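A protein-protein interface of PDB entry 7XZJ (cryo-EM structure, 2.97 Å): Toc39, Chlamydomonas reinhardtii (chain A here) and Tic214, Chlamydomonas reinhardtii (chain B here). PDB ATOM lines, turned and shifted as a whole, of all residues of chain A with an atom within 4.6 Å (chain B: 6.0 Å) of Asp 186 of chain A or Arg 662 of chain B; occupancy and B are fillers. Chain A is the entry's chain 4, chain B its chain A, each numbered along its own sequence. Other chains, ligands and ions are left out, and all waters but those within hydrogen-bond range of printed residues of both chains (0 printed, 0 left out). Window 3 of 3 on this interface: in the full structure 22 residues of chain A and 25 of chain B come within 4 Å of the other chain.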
ATOM      1  N   TYR A 181     -15.183   4.292  16.020  1.00  0.00           N
ATOM      2  CA  TYR A 181     -14.560   3.112  15.366  1.00  0.00           C
ATOM      3  C   TYR A 181     -15.506   1.917  15.490  1.00  0.00           C
ATOM      4  O   TYR A 181     -15.912   1.594  16.623  1.00  0.00           O
ATOM      5  CB  TYR A 181     -13.208   2.783  16.005  1.00  0.00           C
ATOM      6  CG  TYR A 181     -12.680   1.412  15.668  1.00  0.00           C
ATOM      7  CD1 TYR A 181     -12.365   1.066  14.365  1.00  0.00           C
ATOM      8  CD2 TYR A 181     -12.498   0.456  16.653  1.00  0.00           C
ATOM      9  CE1 TYR A 181     -11.885  -0.194  14.047  1.00  0.00           C
ATOM     10  CE2 TYR A 181     -12.017  -0.808  16.354  1.00  0.00           C
ATOM     11  CZ  TYR A 181     -11.709  -1.134  15.045  1.00  0.00           C
ATOM     12  OH  TYR A 181     -11.236  -2.378  14.742  1.00  0.00           O
ATOM     13  N   ASN A 182     -15.849   1.283  14.364  1.00  0.00           N
ATOM     14  CA  ASN A 182     -16.682   0.057  14.441  1.00  0.00           C
ATOM     15  C   ASN A 182     -15.739  -1.141  14.328  1.00  0.00           C
ATOM     16  O   ASN A 182     -15.066  -1.259  13.287  1.00  0.00           O
ATOM     17  CB  ASN A 182     -17.759   0.027  13.356  1.00  0.00           C
ATOM     18  CG  ASN A 182     -18.957  -0.810  13.749  1.00  0.00           C
ATOM     19  OD1 ASN A 182     -19.236  -0.981  14.933  1.00  0.00           O
ATOM     20  ND2 ASN A 182     -19.674  -1.328  12.765  1.00  0.00           N
ATOM     21  N   ASP A 183     -15.688  -1.982  15.362  1.00  0.00           N
ATOM     22  CA  ASP A 183     -14.732  -3.122  15.366  1.00  0.00           C
ATOM     23  C   ASP A 183     -15.067  -4.100  14.237  1.00  0.00           C
ATOM     24  O   ASP A 183     -14.127  -4.550  13.561  1.00  0.00           O
ATOM     25  CB  ASP A 183     -14.681  -3.805  16.735  1.00  0.00           C
ATOM     26  CG  ASP A 183     -16.034  -4.285  17.235  1.00  0.00           C
ATOM     27  OD1 ASP A 183     -16.924  -3.433  17.431  1.00  0.00           O
ATOM     28  OD2 ASP A 183     -16.186  -5.507  17.420  1.00  0.00           O
ATOM     29  N   GLU A 184     -16.353  -4.406  14.032  1.00  0.00           N
ATOM     30  CA  GLU A 184     -16.735  -5.417  13.010  1.00  0.00           C
ATOM     31  C   GLU A 184     -16.315  -4.916  11.626  1.00  0.00           C
ATOM     32  O   GLU A 184     -15.742  -5.712  10.859  1.00  0.00           O
ATOM     33  CB  GLU A 184     -18.243  -5.673  13.052  1.00  0.00           C
ATOM     34  CG  GLU A 184     -18.733  -6.220  14.381  1.00  0.00           C
ATOM     35  CD  GLU A 184     -19.163  -5.172  15.392  1.00  0.00           C
ATOM     36  OE1 GLU A 184     -19.135  -3.976  15.049  1.00  0.00           O
ATOM     37  OE2 GLU A 184     -19.525  -5.555  16.521  1.00  0.00           O
ATOM     38  N   THR A 185     -16.575  -3.642  11.326  1.00  0.00           N
ATOM     39  CA  THR A 185     -16.156  -3.062  10.023  1.00  0.00           C
ATOM     40  C   THR A 185     -14.627  -2.985   9.988  1.00  0.00           C
ATOM     41  O   THR A 185     -14.069  -3.065   8.875  1.00  0.00           O
ATOM     42  CB  THR A 185     -16.796  -1.683   9.815  1.00  0.00           C
ATOM     43  OG1 THR A 185     -18.159  -1.766  10.232  1.00  0.00           O
ATOM     44  CG2 THR A 185     -16.730  -1.206   8.381  1.00  0.00           C
ATOM     45  N   ASP A 186     -13.988  -2.832  11.153  1.00  0.00           N
ATOM     46  CA  ASP A 186     -12.505  -2.697  11.238  1.00  0.00           C
ATOM     47  C   ASP A 186     -12.089  -1.407  10.525  1.00  0.00           C
ATOM     48  O   ASP A 186     -10.932  -1.332  10.066  1.00  0.00           O
ATOM     49  CB  ASP A 186     -11.777  -3.951  10.742  1.00  0.00           C
ATOM     50  CG  ASP A 186     -10.392  -4.128  11.342  1.00  0.00           C
ATOM     51  OD1 ASP A 186     -10.078  -3.410  12.312  1.00  0.00           O
ATOM     52  OD2 ASP A 186      -9.638  -4.979  10.831  1.00  0.00           O
ATOM     53  N   LEU A 187     -12.995  -0.426  10.455  1.00  0.00           N
ATOM     54  CA  LEU A 187     -12.698   0.876   9.800  1.00  0.00           C
ATOM     55  C   LEU A 187     -13.303   1.985  10.665  1.00  0.00           C
ATOM     56  O   LEU A 187     -14.263   1.692  11.404  1.00  0.00           O
ATOM     57  CB  LEU A 187     -13.329   0.894   8.404  1.00  0.00           C
ATOM     58  CG  LEU A 187     -12.748  -0.085   7.385  1.00  0.00           C
ATOM     59  CD1 LEU A 187     -13.570  -0.083   6.107  1.00  0.00           C
ATOM     60  CD2 LEU A 187     -11.295   0.245   7.081  1.00  0.00           C
ATOM     61  N   LYS B 657      -3.276   6.411  12.854  1.00  0.00           N
ATOM     62  CA  LYS B 657      -2.990   6.907  11.513  1.00  0.00           C
ATOM     63  C   LYS B 657      -3.215   5.820  10.470  1.00  0.00           C
ATOM     64  O   LYS B 657      -3.802   6.076   9.411  1.00  0.00           O
ATOM     65  CB  LYS B 657      -1.559   7.438  11.441  1.00  0.00           C
ATOM     66  N   LEU B 658      -2.768   4.596  10.759  1.00  0.00           N
ATOM     67  CA  LEU B 658      -2.991   3.489   9.836  1.00  0.00           C
ATOM     68  C   LEU B 658      -4.477   3.205   9.666  1.00  0.00           C
ATOM     69  O   LEU B 658      -4.940   2.930   8.555  1.00  0.00           O
ATOM     70  CB  LEU B 658      -2.266   2.238  10.329  1.00  0.00           C
ATOM     71  CG  LEU B 658      -0.741   2.295  10.328  1.00  0.00           C
ATOM     72  CD1 LEU B 658      -0.168   1.017  10.912  1.00  0.00           C
ATOM     73  CD2 LEU B 658      -0.215   2.529   8.923  1.00  0.00           C
ATOM     74  N   LEU B 659      -5.237   3.249  10.762  1.00  0.00           N
ATOM     75  CA  LEU B 659      -6.669   2.989  10.675  1.00  0.00           C
ATOM     76  C   LEU B 659      -7.375   4.053   9.843  1.00  0.00           C
ATOM     77  O   LEU B 659      -8.229   3.734   9.004  1.00  0.00           O
ATOM     78  CB  LEU B 659      -7.264   2.917  12.079  1.00  0.00           C
ATOM     79  CG  LEU B 659      -8.528   2.077  12.232  1.00  0.00           C
ATOM     80  CD1 LEU B 659      -8.325   0.702  11.624  1.00  0.00           C
ATOM     81  CD2 LEU B 659      -8.868   1.962  13.701  1.00  0.00           C
ATOM     82  N   GLU B 660      -7.022   5.324  10.056  1.00  0.00           N
ATOM     83  CA  GLU B 660      -7.603   6.396   9.255  1.00  0.00           C
ATOM     84  C   GLU B 660      -7.236   6.240   7.787  1.00  0.00           C
ATOM     85  O   GLU B 660      -8.079   6.439   6.902  1.00  0.00           O
ATOM     86  CB  GLU B 660      -7.145   7.757   9.784  1.00  0.00           C
ATOM     87  N   LEU B 661      -5.978   5.875   7.525  1.00  0.00           N
ATOM     88  CA  LEU B 661      -5.515   5.697   6.123  1.00  0.00           C
ATOM     89  C   LEU B 661      -6.261   4.515   5.499  1.00  0.00           C
ATOM     90  O   LEU B 661      -6.705   4.647   4.346  1.00  0.00           O
ATOM     91  CB  LEU B 661      -4.004   5.450   6.124  1.00  0.00           C
ATOM     92  N   ARG B 662      -6.404   3.415   6.243  1.00  0.00           N
ATOM     93  CA  ARG B 662      -7.073   2.199   5.711  1.00  0.00           C
ATOM     94  C   ARG B 662      -8.525   2.545   5.372  1.00  0.00           C
ATOM     95  O   ARG B 662      -9.009   2.099   4.316  1.00  0.00           O
ATOM     96  CB  ARG B 662      -7.032   1.087   6.763  1.00  0.00           C
ATOM     97  CG  ARG B 662      -7.500  -0.275   6.271  1.00  0.00           C
ATOM     98  CD  ARG B 662      -7.744  -1.217   7.434  1.00  0.00           C
ATOM     99  NE  ARG B 662      -6.617  -1.265   8.353  1.00  0.00           N
ATOM    100  CZ  ARG B 662      -6.604  -1.948   9.492  1.00  0.00           C
ATOM    101  NH1 ARG B 662      -7.668  -2.643   9.858  1.00  0.00           N
ATOM    102  NH2 ARG B 662      -5.531  -1.932  10.262  1.00  0.00           N
ATOM    103  N   THR B 663      -9.179   3.322   6.237  1.00  0.00           N
ATOM    104  CA  THR B 663     -10.583   3.729   5.985  1.00  0.00           C
ATOM    105  C   THR B 663     -10.630   4.601   4.728  1.00  0.00           C
ATOM    106  O   THR B 663     -11.360   4.232   3.785  1.00  0.00           O
ATOM    107  CB  THR B 663     -11.176   4.477   7.183  1.00  0.00           C
ATOM    108  OG1 THR B 663     -10.969   3.681   8.350  1.00  0.00           O
ATOM    109  CG2 THR B 663     -12.649   4.767   7.006  1.00  0.00           C
ATOM    110  N   GLN B 664      -9.883   5.711   4.724  1.00  0.00           N
ATOM    111  CA  GLN B 664      -9.893   6.600   3.567  1.00  0.00           C
ATOM    112  C   GLN B 664      -9.665   5.826   2.275  1.00  0.00           C
ATOM    113  O   GLN B 664     -10.284   6.125   1.248  1.00  0.00           O
ATOM    114  CB  GLN B 664      -8.836   7.691   3.733  1.00  0.00           C
ATOM    115  N   TYR B 665      -8.787   4.821   2.312  1.00  0.00           N
ATOM    116  CA  TYR B 665      -8.428   4.099   1.098  1.00  0.00           C
ATOM    117  C   TYR B 665      -9.562   3.201   0.624  1.00  0.00           C
ATOM    118  O   TYR B 665      -9.815   3.101  -0.581  1.00  0.00           O
ATOM    119  CB  TYR B 665      -7.162   3.275   1.335  1.00  0.00           C
ATOM    120  N   ASN B 666     -10.248   2.534   1.553  1.00  0.00           N
ATOM    121  CA  ASN B 666     -11.274   1.578   1.151  1.00  0.00           C
ATOM    122  C   ASN B 666     -12.382   2.255   0.353  1.00  0.00           C
ATOM    123  O   ASN B 666     -12.894   1.684  -0.616  1.00  0.00           O
ATOM    124  CB  ASN B 666     -11.845   0.870   2.378  1.00  0.00           C
ATOM    125  CG  ASN B 666     -12.748  -0.293   2.005  1.00  0.00           C
ATOM    126  OD1 ASN B 666     -13.785  -0.518   2.630  1.00  0.00           O
ATOM    127  ND2 ASN B 666     -12.365  -1.027   0.967  1.00  0.00           N
ATOM    128  N   ASN B 667     -12.765   3.465   0.742  1.00  0.00           N
ATOM    129  CA  ASN B 667     -13.792   4.209   0.023  1.00  0.00           C
ATOM    130  C   ASN B 667     -13.167   5.138  -1.010  1.00  0.00           C
ATOM    131  O   ASN B 667     -12.327   4.723  -1.806  1.00  0.00           O
ATOM    132  CB  ASN B 667     -14.670   5.000   0.992  1.00  0.00           C
ATOM    133  CG  ASN B 667     -15.591   4.111   1.805  1.00  0.00           C
ATOM    134  OD1 ASN B 667     -15.906   2.991   1.402  1.00  0.00           O
ATOM    135  ND2 ASN B 667     -16.028   4.605   2.958  1.00  0.00           N
ATOM    136  N   ALA B1971       0.003  -6.662  13.508  1.00  0.00           N
ATOM    137  CA  ALA B1971      -0.887  -6.092  12.470  1.00  0.00           C
ATOM    138  C   ALA B1971      -1.526  -4.797  12.979  1.00  0.00           C
ATOM    139  O   ALA B1971      -2.399  -4.263  12.266  1.00  0.00           O
ATOM    140  CB  ALA B1971      -1.935  -7.104  12.084  1.00  0.00           C
ATOM    141  N   TYR B1972      -1.131  -4.334  14.170  1.00  0.00           N
ATOM    142  CA  TYR B1972      -1.750  -3.125  14.773  1.00  0.00           C
ATOM    143  C   TYR B1972      -3.263  -3.344  14.855  1.00  0.00           C
ATOM    144  O   TYR B1972      -4.017  -2.369  14.698  1.00  0.00           O
ATOM    145  CB  TYR B1972      -1.386  -1.866  13.982  1.00  0.00           C
ATOM    146  CG  TYR B1972       0.049  -1.426  14.114  1.00  0.00           C
ATOM    147  CD1 TYR B1972       0.424  -0.492  15.065  1.00  0.00           C
ATOM    148  CD2 TYR B1972       1.035  -1.937  13.286  1.00  0.00           C
ATOM    149  CE1 TYR B1972       1.739  -0.078  15.193  1.00  0.00           C
ATOM    150  CE2 TYR B1972       2.355  -1.535  13.400  1.00  0.00           C
ATOM    151  CZ  TYR B1972       2.709  -0.602  14.358  1.00  0.00           C
ATOM    152  OH  TYR B1972       4.008  -0.200  14.477  1.00  0.00           O
ATOM    153  N   SER B1973      -3.682  -4.592  15.076  1.00  0.00           N
ATOM    154  CA  SER B1973      -5.126  -4.923  15.191  1.00  0.00           C
ATOM    155  C   SER B1973      -5.445  -5.177  16.665  1.00  0.00           C
ATOM    156  O   SER B1973      -6.400  -5.925  16.943  1.00  0.00           O
ATOM    157  CB  SER B1973      -5.483  -6.100  14.328  1.00  0.00           C
ATOM    158  OG  SER B1973      -5.172  -5.837  12.968  1.00  0.00           O
ATOM    159  N   GLN B1975      -6.797  -3.352  18.705  1.00  0.00           N
ATOM    160  CA  GLN B1975      -8.168  -2.861  19.002  1.00  0.00           C
ATOM    161  C   GLN B1975      -9.161  -4.022  18.869  1.00  0.00           C
ATOM    162  O   GLN B1975     -10.089  -4.094  19.696  1.00  0.00           O
ATOM    163  CB  GLN B1975      -8.521  -1.692  18.077  1.00  0.00           C
ATOM    164  CG  GLN B1975      -8.395  -1.997  16.590  1.00  0.00           C
ATOM    165  CD  GLN B1975      -7.042  -1.656  16.016  1.00  0.00           C
ATOM    166  OE1 GLN B1975      -6.098  -1.348  16.738  1.00  0.00           O
ATOM    167  NE2 GLN B1975      -6.940  -1.710  14.698  1.00  0.00           N
ATOM    168  N   GLN B1976      -8.973  -4.896  17.874  1.00  0.00           N
ATOM    169  CA  GLN B1976      -9.910  -6.028  17.638  1.00  0.00           C
ATOM    170  C   GLN B1976      -9.377  -7.237  18.417  1.00  0.00           C
ATOM    171  O   GLN B1976     -10.021  -8.299  18.354  1.00  0.00           O
ATOM    172  CB  GLN B1976     -10.032  -6.297  16.137  1.00  0.00           C
ATOM    173  CG  GLN B1976     -11.445  -6.636  15.689  1.00  0.00           C
ATOM    174  CD  GLN B1976     -11.523  -6.860  14.199  1.00  0.00           C
ATOM    175  OE1 GLN B1976     -10.525  -6.769  13.487  1.00  0.00           O
ATOM    176  NE2 GLN B1976     -12.717  -7.158  13.715  1.00  0.00           N
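The side-chain amide nitrogen (NE2) of Gln 1976 of chain B lies within hydrogen-bond range of the backbone carbonyl oxygen (O) of Asp 183 of chain A (3.0 Å). OD2 of Asp 186 of chain A is in salt-bridge range of NH1 of Arg 662 of chain B (3.2 Å). OD2 of Asp 186 of chain A sits close to OE1 of Gln 1976 of chain B (3.3 Å).
The side-chain carboxylate of Asp 186 of chain A sits at hydrogen-bond distance from the side-chain hydroxyl of Tyr 181 of chain A, 2.9 Å away. N of Asn 182 of chain A lies within hydrogen-bond range of O of Leu 187 of chain A (3.4 Å). O of Leu 659 of chain B lies within hydrogen-bond range of OG1 of Thr 663 of chain B (2.8 Å). O of Tyr 1972 of chain B is in hydrogen-bond range of NE2 of Gln 1975 of chain B (3.0 Å).
Among the printed residues, merely in contact across the chains: Tyr 181 of chain A with Leu 659 of chain B (3.7 Å), Tyr 181 of chain A with Gln 1975 of chain B (3.4 Å), Asp 186 of chain A with Leu 659 of chain B (3.7 Å), Leu 187 of chain A with Arg 662 of chain B (3.9 Å), Leu 187 of chain A with Thr 663 of chain B (3.6 Å) and Leu 187 of chain A with Asn 666 of chain B (3.5 Å).
Of chain B, only Leu 659 (3.7 Å), Arg 662 (3.2 Å) and Gln 1976 (3.3 Å) come within 4 Å of Asp 186 of chain A. Printed residues of chain B within 4 Å of Leu 187 of chain A: Arg 662, Thr 663 and Asn 666. Of the printed residues of chain A, Leu 659 of chain B touches Tyr 181 (3.7 Å) and Asp 186 (3.7 Å). Of chain A, only Asp 186 (3.2 Å) and Leu 187 (3.9 Å) come within 4 Å of Arg 662 of chain B. Printed residues of chain A within 4 Å of Thr 663 of chain B: Leu 187. Of the printed residues of chain A, Gln 1975 of chain B touches Tyr 181. Of the printed residues of chain A, Gln 1976 of chain B touches Asp 183 (3.0 Å) and Asp 186 (3.3 Å). The nearest printed residue of chain A that does not touch Gln 1975 of chain B is Asp 186 of chain A (4.3 Å).
Printed residues of chain A that touch a printed residue of chain B: Tyr 181, Asp 183, Asp 186 and Leu 187. Hydrophobic or aromatic side chains of chain A that line the printed part of chain B: Tyr 181 and Leu 187. Among the printed residues, Asp or Glu carboxylates within 4 Å of a Lys or Arg side-chain nitrogen of the other chain: Asp 186 of chain A with Arg 662 of chain B.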
